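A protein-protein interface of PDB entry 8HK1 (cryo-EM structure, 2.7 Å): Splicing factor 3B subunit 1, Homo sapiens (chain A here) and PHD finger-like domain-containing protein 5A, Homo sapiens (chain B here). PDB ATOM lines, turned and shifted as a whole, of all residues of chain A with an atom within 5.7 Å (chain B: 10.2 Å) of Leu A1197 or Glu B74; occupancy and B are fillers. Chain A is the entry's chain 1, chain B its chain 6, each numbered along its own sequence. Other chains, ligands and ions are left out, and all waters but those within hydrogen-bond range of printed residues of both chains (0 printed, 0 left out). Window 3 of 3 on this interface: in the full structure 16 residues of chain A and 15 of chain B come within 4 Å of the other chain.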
ATOM      1  N   GLU A1156     -16.228 -21.563 -23.956  1.00  0.00           N
ATOM      2  CA  GLU A1156     -15.258 -22.519 -24.484  1.00  0.00           C
ATOM      3  C   GLU A1156     -15.918 -23.541 -25.406  1.00  0.00           C
ATOM      4  O   GLU A1156     -15.295 -24.023 -26.358  1.00  0.00           O
ATOM      5  CB  GLU A1156     -14.542 -23.228 -23.337  1.00  0.00           C
ATOM      6  CG  GLU A1156     -13.392 -24.106 -23.783  1.00  0.00           C
ATOM      7  CD  GLU A1156     -12.816 -24.931 -22.654  1.00  0.00           C
ATOM      8  OE1 GLU A1156     -13.320 -24.825 -21.518  1.00  0.00           O
ATOM      9  OE2 GLU A1156     -11.854 -25.686 -22.903  1.00  0.00           O
ATOM     10  N   VAL A1192     -12.658 -14.763 -19.798  1.00  0.00           N
ATOM     11  CA  VAL A1192     -12.034 -13.848 -20.755  1.00  0.00           C
ATOM     12  C   VAL A1192     -11.155 -14.614 -21.734  1.00  0.00           C
ATOM     13  O   VAL A1192     -11.167 -14.348 -22.939  1.00  0.00           O
ATOM     14  CB  VAL A1192     -11.240 -12.755 -20.013  1.00  0.00           C
ATOM     15  CG1 VAL A1192     -10.324 -12.020 -20.971  1.00  0.00           C
ATOM     16  CG2 VAL A1192     -12.186 -11.773 -19.355  1.00  0.00           C
ATOM     17  N   GLN A1193     -10.392 -15.589 -21.234  1.00  0.00           N
ATOM     18  CA  GLN A1193      -9.516 -16.366 -22.107  1.00  0.00           C
ATOM     19  C   GLN A1193     -10.316 -17.166 -23.132  1.00  0.00           C
ATOM     20  O   GLN A1193      -9.999 -17.158 -24.333  1.00  0.00           O
ATOM     21  CB  GLN A1193      -8.639 -17.298 -21.273  1.00  0.00           C
ATOM     22  CG  GLN A1193      -7.868 -18.311 -22.101  1.00  0.00           C
ATOM     23  CD  GLN A1193      -7.393 -19.495 -21.290  1.00  0.00           C
ATOM     24  OE1 GLN A1193      -6.883 -19.341 -20.184  1.00  0.00           O
ATOM     25  NE2 GLN A1193      -7.552 -20.687 -21.843  1.00  0.00           N
ATOM     26  N   HIS A1194     -11.354 -17.875 -22.676  1.00  0.00           N
ATOM     27  CA  HIS A1194     -12.131 -18.688 -23.607  1.00  0.00           C
ATOM     28  C   HIS A1194     -12.875 -17.821 -24.612  1.00  0.00           C
ATOM     29  O   HIS A1194     -12.953 -18.161 -25.798  1.00  0.00           O
ATOM     30  CB  HIS A1194     -13.100 -19.595 -22.848  1.00  0.00           C
ATOM     31  CG  HIS A1194     -12.424 -20.610 -21.984  1.00  0.00           C
ATOM     32  ND1 HIS A1194     -12.681 -20.731 -20.637  1.00  0.00           N
ATOM     33  CD2 HIS A1194     -11.487 -21.542 -22.274  1.00  0.00           C
ATOM     34  CE1 HIS A1194     -11.935 -21.698 -20.134  1.00  0.00           C
ATOM     35  NE2 HIS A1194     -11.202 -22.209 -21.107  1.00  0.00           N
ATOM     36  N   MET A1195     -13.408 -16.683 -24.163  1.00  0.00           N
ATOM     37  CA  MET A1195     -14.084 -15.759 -25.066  1.00  0.00           C
ATOM     38  C   MET A1195     -13.116 -15.185 -26.095  1.00  0.00           C
ATOM     39  O   MET A1195     -13.469 -15.039 -27.270  1.00  0.00           O
ATOM     40  CB  MET A1195     -14.737 -14.643 -24.256  1.00  0.00           C
ATOM     41  CG  MET A1195     -16.101 -14.218 -24.746  1.00  0.00           C
ATOM     42  SD  MET A1195     -17.026 -13.370 -23.455  1.00  0.00           S
ATOM     43  CE  MET A1195     -15.942 -11.990 -23.128  1.00  0.00           C
ATOM     44  N   SER A1196     -11.896 -14.853 -25.669  1.00  0.00           N
ATOM     45  CA  SER A1196     -10.904 -14.302 -26.586  1.00  0.00           C
ATOM     46  C   SER A1196     -10.534 -15.311 -27.659  1.00  0.00           C
ATOM     47  O   SER A1196     -10.485 -14.980 -28.846  1.00  0.00           O
ATOM     48  CB  SER A1196      -9.660 -13.869 -25.812  1.00  0.00           C
ATOM     49  OG  SER A1196      -9.739 -12.505 -25.451  1.00  0.00           O
ATOM     50  N   LEU A1197     -10.251 -16.551 -27.257  1.00  0.00           N
ATOM     51  CA  LEU A1197      -9.861 -17.549 -28.246  1.00  0.00           C
ATOM     52  C   LEU A1197     -11.055 -18.013 -29.074  1.00  0.00           C
ATOM     53  O   LEU A1197     -10.882 -18.582 -30.158  1.00  0.00           O
ATOM     54  CB  LEU A1197      -9.167 -18.719 -27.558  1.00  0.00           C
ATOM     55  CG  LEU A1197      -7.774 -18.309 -27.074  1.00  0.00           C
ATOM     56  CD1 LEU A1197      -7.165 -19.339 -26.148  1.00  0.00           C
ATOM     57  CD2 LEU A1197      -6.856 -18.045 -28.258  1.00  0.00           C
ATOM     58  N   GLY A1198     -12.273 -17.776 -28.588  1.00  0.00           N
ATOM     59  CA  GLY A1198     -13.449 -18.154 -29.357  1.00  0.00           C
ATOM     60  C   GLY A1198     -13.735 -17.205 -30.503  1.00  0.00           C
ATOM     61  O   GLY A1198     -14.061 -17.637 -31.611  1.00  0.00           O
ATOM     62  N   VAL A1199     -13.628 -15.906 -30.258  1.00  0.00           N
ATOM     63  CA  VAL A1199     -13.825 -14.893 -31.296  1.00  0.00           C
ATOM     64  C   VAL A1199     -12.435 -14.404 -31.692  1.00  0.00           C
ATOM     65  O   VAL A1199     -11.684 -13.843 -30.895  1.00  0.00           O
ATOM     66  CB  VAL A1199     -14.753 -13.765 -30.833  1.00  0.00           C
ATOM     67  CG1 VAL A1199     -16.088 -14.336 -30.389  1.00  0.00           C
ATOM     68  CG2 VAL A1199     -14.149 -12.961 -29.697  1.00  0.00           C
ATOM     69  N   TYR A1200     -12.065 -14.650 -32.943  1.00  0.00           N
ATOM     70  CA  TYR A1200     -10.737 -14.308 -33.436  1.00  0.00           C
ATOM     71  C   TYR A1200     -10.835 -14.170 -34.945  1.00  0.00           C
ATOM     72  O   TYR A1200     -11.043 -15.162 -35.649  1.00  0.00           O
ATOM     73  CB  TYR A1200      -9.714 -15.373 -33.018  1.00  0.00           C
ATOM     74  CG  TYR A1200      -8.419 -15.392 -33.803  1.00  0.00           C
ATOM     75  CD1 TYR A1200      -7.706 -14.226 -34.043  1.00  0.00           C
ATOM     76  CD2 TYR A1200      -7.896 -16.588 -34.275  1.00  0.00           C
ATOM     77  CE1 TYR A1200      -6.523 -14.246 -34.751  1.00  0.00           C
ATOM     78  CE2 TYR A1200      -6.715 -16.618 -34.981  1.00  0.00           C
ATOM     79  CZ  TYR A1200      -6.032 -15.447 -35.216  1.00  0.00           C
ATOM     80  OH  TYR A1200      -4.854 -15.479 -35.920  1.00  0.00           O
ATOM     81  N   GLU A1235      -2.561 -14.596 -22.603  1.00  0.00           N
ATOM     82  CA  GLU A1235      -2.119 -15.255 -23.828  1.00  0.00           C
ATOM     83  C   GLU A1235      -3.267 -15.439 -24.815  1.00  0.00           C
ATOM     84  O   GLU A1235      -3.043 -15.497 -26.027  1.00  0.00           O
ATOM     85  CB  GLU A1235      -1.455 -16.589 -23.504  1.00  0.00           C
ATOM     86  CG  GLU A1235       0.067 -16.524 -23.519  1.00  0.00           C
ATOM     87  CD  GLU A1235       0.615 -15.559 -24.568  1.00  0.00           C
ATOM     88  OE1 GLU A1235       0.853 -14.375 -24.238  1.00  0.00           O
ATOM     89  OE2 GLU A1235       0.811 -15.983 -25.725  1.00  0.00           O
ATOM     90  N   GLY A1236      -4.503 -15.530 -24.319  1.00  0.00           N
ATOM     91  CA  GLY A1236      -5.643 -15.486 -25.222  1.00  0.00           C
ATOM     92  C   GLY A1236      -5.854 -14.122 -25.847  1.00  0.00           C
ATOM     93  O   GLY A1236      -6.175 -14.022 -27.040  1.00  0.00           O
ATOM     94  N   VAL A1239      -3.669 -13.330 -28.838  1.00  0.00           N
ATOM     95  CA  VAL A1239      -4.143 -13.793 -30.136  1.00  0.00           C
ATOM     96  C   VAL A1239      -5.315 -12.947 -30.613  1.00  0.00           C
ATOM     97  O   VAL A1239      -5.363 -12.531 -31.776  1.00  0.00           O
ATOM     98  CB  VAL A1239      -4.511 -15.289 -30.067  1.00  0.00           C
ATOM     99  CG1 VAL A1239      -5.145 -15.743 -31.369  1.00  0.00           C
ATOM    100  CG2 VAL A1239      -3.281 -16.121 -29.754  1.00  0.00           C
ATOM    101  N   ALA A1240      -6.272 -12.670 -29.729  1.00  0.00           N
ATOM    102  CA  ALA A1240      -7.501 -12.013 -30.176  1.00  0.00           C
ATOM    103  C   ALA A1240      -7.307 -10.513 -30.398  1.00  0.00           C
ATOM    104  O   ALA A1240      -7.954  -9.914 -31.262  1.00  0.00           O
ATOM    105  CB  ALA A1240      -8.624 -12.263 -29.166  1.00  0.00           C
ATOM    106  N   CYS B  30      -6.964 -33.643 -23.860  1.00  0.00           N
ATOM    107  CA  CYS B  30      -5.847 -32.934 -24.464  1.00  0.00           C
ATOM    108  C   CYS B  30      -4.646 -32.998 -23.523  1.00  0.00           C
ATOM    109  O   CYS B  30      -4.763 -32.824 -22.311  1.00  0.00           O
ATOM    110  CB  CYS B  30      -6.239 -31.491 -24.779  1.00  0.00           C
ATOM    111  SG  CYS B  30      -4.867 -30.409 -25.260  1.00  0.00           S
ATOM    112  N   ILE B  32      -2.009 -31.121 -23.106  1.00  0.00           N
ATOM    113  CA  ILE B  32      -1.377 -29.911 -22.593  1.00  0.00           C
ATOM    114  C   ILE B  32      -2.285 -29.194 -21.601  1.00  0.00           C
ATOM    115  O   ILE B  32      -1.833 -28.763 -20.534  1.00  0.00           O
ATOM    116  CB  ILE B  32      -0.970 -28.985 -23.752  1.00  0.00           C
ATOM    117  CG1 ILE B  32       0.184 -29.607 -24.537  1.00  0.00           C
ATOM    118  CG2 ILE B  32      -0.587 -27.606 -23.234  1.00  0.00           C
ATOM    119  CD1 ILE B  32       0.931 -28.633 -25.402  1.00  0.00           C
ATOM    120  N   CYS B  33      -3.569 -29.065 -21.931  1.00  0.00           N
ATOM    121  CA  CYS B  33      -4.477 -28.292 -21.093  1.00  0.00           C
ATOM    122  C   CYS B  33      -5.565 -29.134 -20.435  1.00  0.00           C
ATOM    123  O   CYS B  33      -6.310 -28.601 -19.607  1.00  0.00           O
ATOM    124  CB  CYS B  33      -5.125 -27.169 -21.908  1.00  0.00           C
ATOM    125  SG  CYS B  33      -6.298 -27.715 -23.161  1.00  0.00           S
ATOM    126  N   ASP B  34      -5.690 -30.412 -20.806  1.00  0.00           N
ATOM    127  CA  ASP B  34      -6.625 -31.349 -20.176  1.00  0.00           C
ATOM    128  C   ASP B  34      -8.077 -31.004 -20.499  1.00  0.00           C
ATOM    129  O   ASP B  34      -8.992 -31.274 -19.721  1.00  0.00           O
ATOM    130  CB  ASP B  34      -6.405 -31.429 -18.661  1.00  0.00           C
ATOM    131  CG  ASP B  34      -5.236 -32.315 -18.287  1.00  0.00           C
ATOM    132  OD1 ASP B  34      -5.353 -33.074 -17.302  1.00  0.00           O
ATOM    133  OD2 ASP B  34      -4.199 -32.255 -18.979  1.00  0.00           O
ATOM    134  N   SER B  35      -8.288 -30.412 -21.668  1.00  0.00           N
ATOM    135  CA  SER B  35      -9.629 -30.091 -22.132  1.00  0.00           C
ATOM    136  C   SER B  35     -10.217 -31.298 -22.857  1.00  0.00           C
ATOM    137  O   SER B  35      -9.502 -32.216 -23.265  1.00  0.00           O
ATOM    138  CB  SER B  35      -9.601 -28.854 -23.026  1.00  0.00           C
ATOM    139  OG  SER B  35     -10.911 -28.411 -23.334  1.00  0.00           O
ATOM    140  N   TYR B  36     -11.543 -31.308 -23.023  1.00  0.00           N
ATOM    141  CA  TYR B  36     -12.183 -32.391 -23.762  1.00  0.00           C
ATOM    142  C   TYR B  36     -12.866 -31.905 -25.034  1.00  0.00           C
ATOM    143  O   TYR B  36     -13.420 -32.731 -25.771  1.00  0.00           O
ATOM    144  CB  TYR B  36     -13.218 -33.114 -22.886  1.00  0.00           C
ATOM    145  CG  TYR B  36     -12.627 -34.132 -21.943  1.00  0.00           C
ATOM    146  CD1 TYR B  36     -12.554 -35.472 -22.298  1.00  0.00           C
ATOM    147  CD2 TYR B  36     -12.143 -33.757 -20.698  1.00  0.00           C
ATOM    148  CE1 TYR B  36     -12.012 -36.408 -21.442  1.00  0.00           C
ATOM    149  CE2 TYR B  36     -11.601 -34.686 -19.834  1.00  0.00           C
ATOM    150  CZ  TYR B  36     -11.537 -36.011 -20.211  1.00  0.00           C
ATOM    151  OH  TYR B  36     -10.998 -36.940 -19.353  1.00  0.00           O
ATOM    152  N   VAL B  37     -12.847 -30.607 -25.321  1.00  0.00           N
ATOM    153  CA  VAL B  37     -13.614 -30.035 -26.421  1.00  0.00           C
ATOM    154  C   VAL B  37     -12.717 -29.868 -27.641  1.00  0.00           C
ATOM    155  O   VAL B  37     -11.560 -29.447 -27.533  1.00  0.00           O
ATOM    156  CB  VAL B  37     -14.281 -28.698 -26.020  1.00  0.00           C
ATOM    157  CG1 VAL B  37     -14.938 -28.828 -24.656  1.00  0.00           C
ATOM    158  CG2 VAL B  37     -13.293 -27.550 -26.012  1.00  0.00           C
ATOM    159  N   ARG B  38     -13.253 -30.255 -28.800  1.00  0.00           N
ATOM    160  CA  ARG B  38     -12.706 -30.039 -30.135  1.00  0.00           C
ATOM    161  C   ARG B  38     -11.251 -30.477 -30.279  1.00  0.00           C
ATOM    162  O   ARG B  38     -10.357 -29.627 -30.377  1.00  0.00           O
ATOM    163  CB  ARG B  38     -12.850 -28.565 -30.518  1.00  0.00           C
ATOM    164  CG  ARG B  38     -13.982 -28.317 -31.496  1.00  0.00           C
ATOM    165  CD  ARG B  38     -14.479 -26.886 -31.441  1.00  0.00           C
ATOM    166  NE  ARG B  38     -13.809 -26.035 -32.417  1.00  0.00           N
ATOM    167  CZ  ARG B  38     -14.310 -24.897 -32.880  1.00  0.00           C
ATOM    168  NH1 ARG B  38     -13.633 -24.184 -33.770  1.00  0.00           N
ATOM    169  NH2 ARG B  38     -15.492 -24.471 -32.453  1.00  0.00           N
ATOM    170  N   PRO B  39     -10.969 -31.784 -30.295  1.00  0.00           N
ATOM    171  CA  PRO B  39      -9.614 -32.235 -30.649  1.00  0.00           C
ATOM    172  C   PRO B  39      -9.268 -31.865 -32.084  1.00  0.00           C
ATOM    173  O   PRO B  39     -10.068 -32.099 -32.994  1.00  0.00           O
ATOM    174  CB  PRO B  39      -9.669 -33.756 -30.457  1.00  0.00           C
ATOM    175  CG  PRO B  39     -10.993 -34.068 -29.871  1.00  0.00           C
ATOM    176  CD  PRO B  39     -11.889 -32.895 -30.009  1.00  0.00           C
ATOM    177  N   CYS B  40      -8.078 -31.287 -32.306  1.00  0.00           N
ATOM    178  CA  CYS B  40      -7.797 -30.719 -33.619  1.00  0.00           C
ATOM    179  C   CYS B  40      -6.541 -31.265 -34.296  1.00  0.00           C
ATOM    180  O   CYS B  40      -6.576 -31.513 -35.505  1.00  0.00           O
ATOM    181  CB  CYS B  40      -7.678 -29.190 -33.505  1.00  0.00           C
ATOM    182  SG  CYS B  40      -6.923 -28.374 -34.925  1.00  0.00           S
ATOM    183  N   THR B  41      -5.445 -31.478 -33.570  1.00  0.00           N
ATOM    184  CA  THR B  41      -4.161 -31.778 -34.188  1.00  0.00           C
ATOM    185  C   THR B  41      -3.564 -33.037 -33.577  1.00  0.00           C
ATOM    186  O   THR B  41      -3.497 -33.185 -32.356  1.00  0.00           O
ATOM    187  CB  THR B  41      -3.175 -30.602 -34.035  1.00  0.00           C
ATOM    188  OG1 THR B  41      -3.632 -29.488 -34.809  1.00  0.00           O
ATOM    189  CG2 THR B  41      -1.784 -30.991 -34.510  1.00  0.00           C
ATOM    190  N   TYR B  70      -4.512 -36.095 -29.228  1.00  0.00           N
ATOM    191  CA  TYR B  70      -4.807 -34.911 -30.023  1.00  0.00           C
ATOM    192  C   TYR B  70      -4.581 -33.653 -29.200  1.00  0.00           C
ATOM    193  O   TYR B  70      -4.782 -33.651 -27.982  1.00  0.00           O
ATOM    194  CB  TYR B  70      -6.252 -34.925 -30.533  1.00  0.00           C
ATOM    195  CG  TYR B  70      -6.472 -35.755 -31.772  1.00  0.00           C
ATOM    196  CD1 TYR B  70      -6.144 -35.262 -33.025  1.00  0.00           C
ATOM    197  CD2 TYR B  70      -7.022 -37.026 -31.689  1.00  0.00           C
ATOM    198  CE1 TYR B  70      -6.347 -36.016 -34.160  1.00  0.00           C
ATOM    199  CE2 TYR B  70      -7.229 -37.786 -32.818  1.00  0.00           C
ATOM    200  CZ  TYR B  70      -6.890 -37.278 -34.051  1.00  0.00           C
ATOM    201  OH  TYR B  70      -7.095 -38.031 -35.180  1.00  0.00           O
ATOM    202  N   TYR B  71      -4.156 -32.588 -29.868  1.00  0.00           N
ATOM    203  CA  TYR B  71      -4.223 -31.253 -29.300  1.00  0.00           C
ATOM    204  C   TYR B  71      -5.607 -30.670 -29.549  1.00  0.00           C
ATOM    205  O   TYR B  71      -6.269 -30.997 -30.535  1.00  0.00           O
ATOM    206  CB  TYR B  71      -3.167 -30.324 -29.903  1.00  0.00           C
ATOM    207  CG  TYR B  71      -1.733 -30.764 -29.731  1.00  0.00           C
ATOM    208  CD1 TYR B  71      -1.066 -30.568 -28.531  1.00  0.00           C
ATOM    209  CD2 TYR B  71      -1.033 -31.341 -30.780  1.00  0.00           C
ATOM    210  CE1 TYR B  71       0.250 -30.954 -28.375  1.00  0.00           C
ATOM    211  CE2 TYR B  71       0.280 -31.729 -30.633  1.00  0.00           C
ATOM    212  CZ  TYR B  71       0.915 -31.531 -29.431  1.00  0.00           C
ATOM    213  OH  TYR B  71       2.227 -31.918 -29.283  1.00  0.00           O
ATOM    214  N   CYS B  72      -6.037 -29.797 -28.649  1.00  0.00           N
ATOM    215  CA  CYS B  72      -7.319 -29.137 -28.818  1.00  0.00           C
ATOM    216  C   CYS B  72      -7.182 -27.939 -29.751  1.00  0.00           C
ATOM    217  O   CYS B  72      -6.085 -27.436 -30.005  1.00  0.00           O
ATOM    218  CB  CYS B  72      -7.879 -28.700 -27.467  1.00  0.00           C
ATOM    219  SG  CYS B  72      -6.974 -27.349 -26.686  1.00  0.00           S
ATOM    220  N   LYS B  73      -8.325 -27.480 -30.272  1.00  0.00           N
ATOM    221  CA  LYS B  73      -8.332 -26.310 -31.140  1.00  0.00           C
ATOM    222  C   LYS B  73      -7.777 -25.077 -30.440  1.00  0.00           C
ATOM    223  O   LYS B  73      -7.134 -24.241 -31.087  1.00  0.00           O
ATOM    224  CB  LYS B  73      -9.755 -26.034 -31.632  1.00  0.00           C
ATOM    225  CG  LYS B  73      -9.848 -25.006 -32.744  1.00  0.00           C
ATOM    226  CD  LYS B  73      -9.058 -25.437 -33.965  1.00  0.00           C
ATOM    227  CE  LYS B  73      -9.842 -26.433 -34.805  1.00  0.00           C
ATOM    228  NZ  LYS B  73     -10.592 -25.770 -35.898  1.00  0.00           N
ATOM    229  N   GLU B  74      -7.975 -24.974 -29.129  1.00  0.00           N
ATOM    230  CA  GLU B  74      -7.474 -23.829 -28.376  1.00  0.00           C
ATOM    231  C   GLU B  74      -5.953 -23.829 -28.313  1.00  0.00           C
ATOM    232  O   GLU B  74      -5.322 -22.774 -28.441  1.00  0.00           O
ATOM    233  CB  GLU B  74      -8.075 -23.847 -26.974  1.00  0.00           C
ATOM    234  CG  GLU B  74      -8.495 -22.504 -26.462  1.00  0.00           C
ATOM    235  CD  GLU B  74      -9.684 -22.588 -25.536  1.00  0.00           C
ATOM    236  OE1 GLU B  74     -10.793 -22.905 -26.011  1.00  0.00           O
ATOM    237  OE2 GLU B  74      -9.512 -22.335 -24.329  1.00  0.00           O
ATOM    238  N   CYS B  75      -5.345 -25.000 -28.109  1.00  0.00           N
ATOM    239  CA  CYS B  75      -3.893 -25.115 -28.117  1.00  0.00           C
ATOM    240  C   CYS B  75      -3.310 -25.009 -29.517  1.00  0.00           C
ATOM    241  O   CYS B  75      -2.164 -24.569 -29.667  1.00  0.00           O
ATOM    242  CB  CYS B  75      -3.461 -26.437 -27.480  1.00  0.00           C
ATOM    243  SG  CYS B  75      -3.387 -26.415 -25.675  1.00  0.00           S
ATOM    244  N   THR B  76      -4.064 -25.405 -30.539  1.00  0.00           N
ATOM    245  CA  THR B  76      -3.599 -25.288 -31.915  1.00  0.00           C
ATOM    246  C   THR B  76      -3.590 -23.833 -32.369  1.00  0.00           C
ATOM    247  O   THR B  76      -2.679 -23.406 -33.083  1.00  0.00           O
ATOM    248  CB  THR B  76      -4.478 -26.138 -32.834  1.00  0.00           C
ATOM    249  OG1 THR B  76      -4.410 -27.507 -32.421  1.00  0.00           O
ATOM    250  CG2 THR B  76      -4.019 -26.030 -34.279  1.00  0.00           C
ATOM    251  N   ILE B  77      -4.594 -23.057 -31.951  1.00  0.00           N
ATOM    252  CA  ILE B  77      -4.625 -21.639 -32.289  1.00  0.00           C
ATOM    253  C   ILE B  77      -3.425 -20.894 -31.714  1.00  0.00           C
ATOM    254  O   ILE B  77      -2.861 -20.025 -32.387  1.00  0.00           O
ATOM    255  CB  ILE B  77      -5.946 -21.008 -31.807  1.00  0.00           C
ATOM    256  CG1 ILE B  77      -7.109 -21.480 -32.675  1.00  0.00           C
ATOM    257  CG2 ILE B  77      -5.866 -19.492 -31.831  1.00  0.00           C
ATOM    258  CD1 ILE B  77      -8.450 -20.962 -32.219  1.00  0.00           C
ATOM    259  N   GLN B  78      -3.005 -21.228 -30.496  1.00  0.00           N
ATOM    260  CA  GLN B  78      -1.864 -20.581 -29.867  1.00  0.00           C
ATOM    261  C   GLN B  78      -0.534 -21.226 -30.240  1.00  0.00           C
ATOM    262  O   GLN B  78       0.497 -20.851 -29.673  1.00  0.00           O
ATOM    263  CB  GLN B  78      -2.030 -20.593 -28.343  1.00  0.00           C
ATOM    264  CG  GLN B  78      -3.346 -20.005 -27.868  1.00  0.00           C
ATOM    265  CD  GLN B  78      -3.612 -20.271 -26.402  1.00  0.00           C
ATOM    266  OE1 GLN B  78      -3.862 -21.407 -26.001  1.00  0.00           O
ATOM    267  NE2 GLN B  78      -3.565 -19.223 -25.592  1.00  0.00           N
ATOM    268  N   GLU B  79      -0.543 -22.185 -31.168  1.00  0.00           N
ATOM    269  CA  GLU B  79       0.667 -22.850 -31.653  1.00  0.00           C
ATOM    270  C   GLU B  79       1.442 -23.517 -30.520  1.00  0.00           C
ATOM    271  O   GLU B  79       2.674 -23.508 -30.496  1.00  0.00           O
ATOM    272  CB  GLU B  79       1.562 -21.885 -32.433  1.00  0.00           C
ATOM    273  CG  GLU B  79       0.903 -21.303 -33.671  1.00  0.00           C
ATOM    274  CD  GLU B  79       1.880 -21.106 -34.814  1.00  0.00           C
ATOM    275  OE1 GLU B  79       3.101 -21.080 -34.560  1.00  0.00           O
ATOM    276  OE2 GLU B  79       1.424 -20.979 -35.969  1.00  0.00           O
ATOM    277  N   LYS B  80       0.719 -24.112 -29.579  1.00  0.00           N
ATOM    278  CA  LYS B  80       1.334 -24.890 -28.516  1.00  0.00           C
ATOM    279  C   LYS B  80       1.648 -26.313 -28.950  1.00  0.00           C
ATOM    280  O   LYS B  80       2.228 -27.073 -28.169  1.00  0.00           O
ATOM    281  CB  LYS B  80       0.432 -24.900 -27.278  1.00  0.00           C
ATOM    282  CG  LYS B  80       0.327 -23.541 -26.609  1.00  0.00           C
ATOM    283  CD  LYS B  80       0.207 -23.656 -25.106  1.00  0.00           C
ATOM    284  CE  LYS B  80      -1.242 -23.640 -24.663  1.00  0.00           C
ATOM    285  NZ  LYS B  80      -1.357 -23.619 -23.182  1.00  0.00           N
ATOM    286  N   ASP B  81       1.273 -26.689 -30.168  1.00  0.00           N
ATOM    287  CA  ASP B  81       1.680 -27.943 -30.782  1.00  0.00           C
ATOM    288  C   ASP B  81       3.045 -27.851 -31.449  1.00  0.00           C
ATOM    289  O   ASP B  81       3.474 -28.814 -32.091  1.00  0.00           O
ATOM    290  CB  ASP B  81       0.636 -28.391 -31.807  1.00  0.00           C
ATOM    291  CG  ASP B  81       0.498 -27.421 -32.965  1.00  0.00           C
ATOM    292  OD1 ASP B  81       0.175 -26.240 -32.722  1.00  0.00           O
ATOM    293  OD2 ASP B  81       0.706 -27.840 -34.121  1.00  0.00           O
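The side-chain carboxylate of Glu A1156 lies within hydrogen-bond range of the side-chain hydroxyl of Ser B35, at 2.9 Å.
SG of Cys B33 sits close to N of Ser B35 (3.7 Å).
The side-chain sulfur (SG) of Cys B72 sits close to the backbone NH (N) of Glu B74 (3.6 Å).
O of Ser B35 is in hydrogen-bond range of N of Cys B30.
OE1 of Glu A1156 is in hydrogen-bond range of NE2 of His A1194 (3.4 Å).
OE1 of Gln B78 lies close to O of Glu B74, at 3.2 Å.
Among the printed residues, merely in contact across the chains: Glu A1156 with Val B37 (3.9 Å), Glu A1156 with Glu B74 (3.6 Å), Gln A1193 with Glu B74 (3.6 Å), His A1194 with Glu B74 (3.0 Å), Leu A1197 with Glu B74 (3.4 Å), Leu A1197 with Ile B77 (3.98 Å), Leu A1197 with Gln B78 (3.6 Å), Glu A1235 with Gln B78 (3.8 Å) and Val A1239 with Ile B77 (3.8 Å).
Glu B74 touches just these residues of chain A: Glu A1156 (3.6 Å), Gln A1193 (3.6 Å), His A1194 (3.0 Å) and Leu A1197 (3.4 Å).
Gln A1193 touches just one residue of chain B: Glu B74 (3.6 Å).
No residue of chain B comes within 4 Å of Ser A1196.
No residue of chain B comes within 4 Å of Gly A1198.
Of the printed residues of chain A, Gln B78 touches Leu A1197 and Glu A1235.
Of the printed residues of chain B, Glu A1235 touches Gln B78 (3.8 Å).
Cys B30 touches none of the printed residues of chain A.
Thr B41 touches none of the printed residues of chain A.
The nearest printed residue of chain A that does not touch Glu B74 is Gly A1198 (5.9 Å).
The nearest printed residue of chain A that does not touch Ile B77 is Tyr A1200 (4.3 Å).
Among the printed residues, no Asp or Glu carboxylate lies within 4 Å of a Lys or Arg side-chain nitrogen of the other chain.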
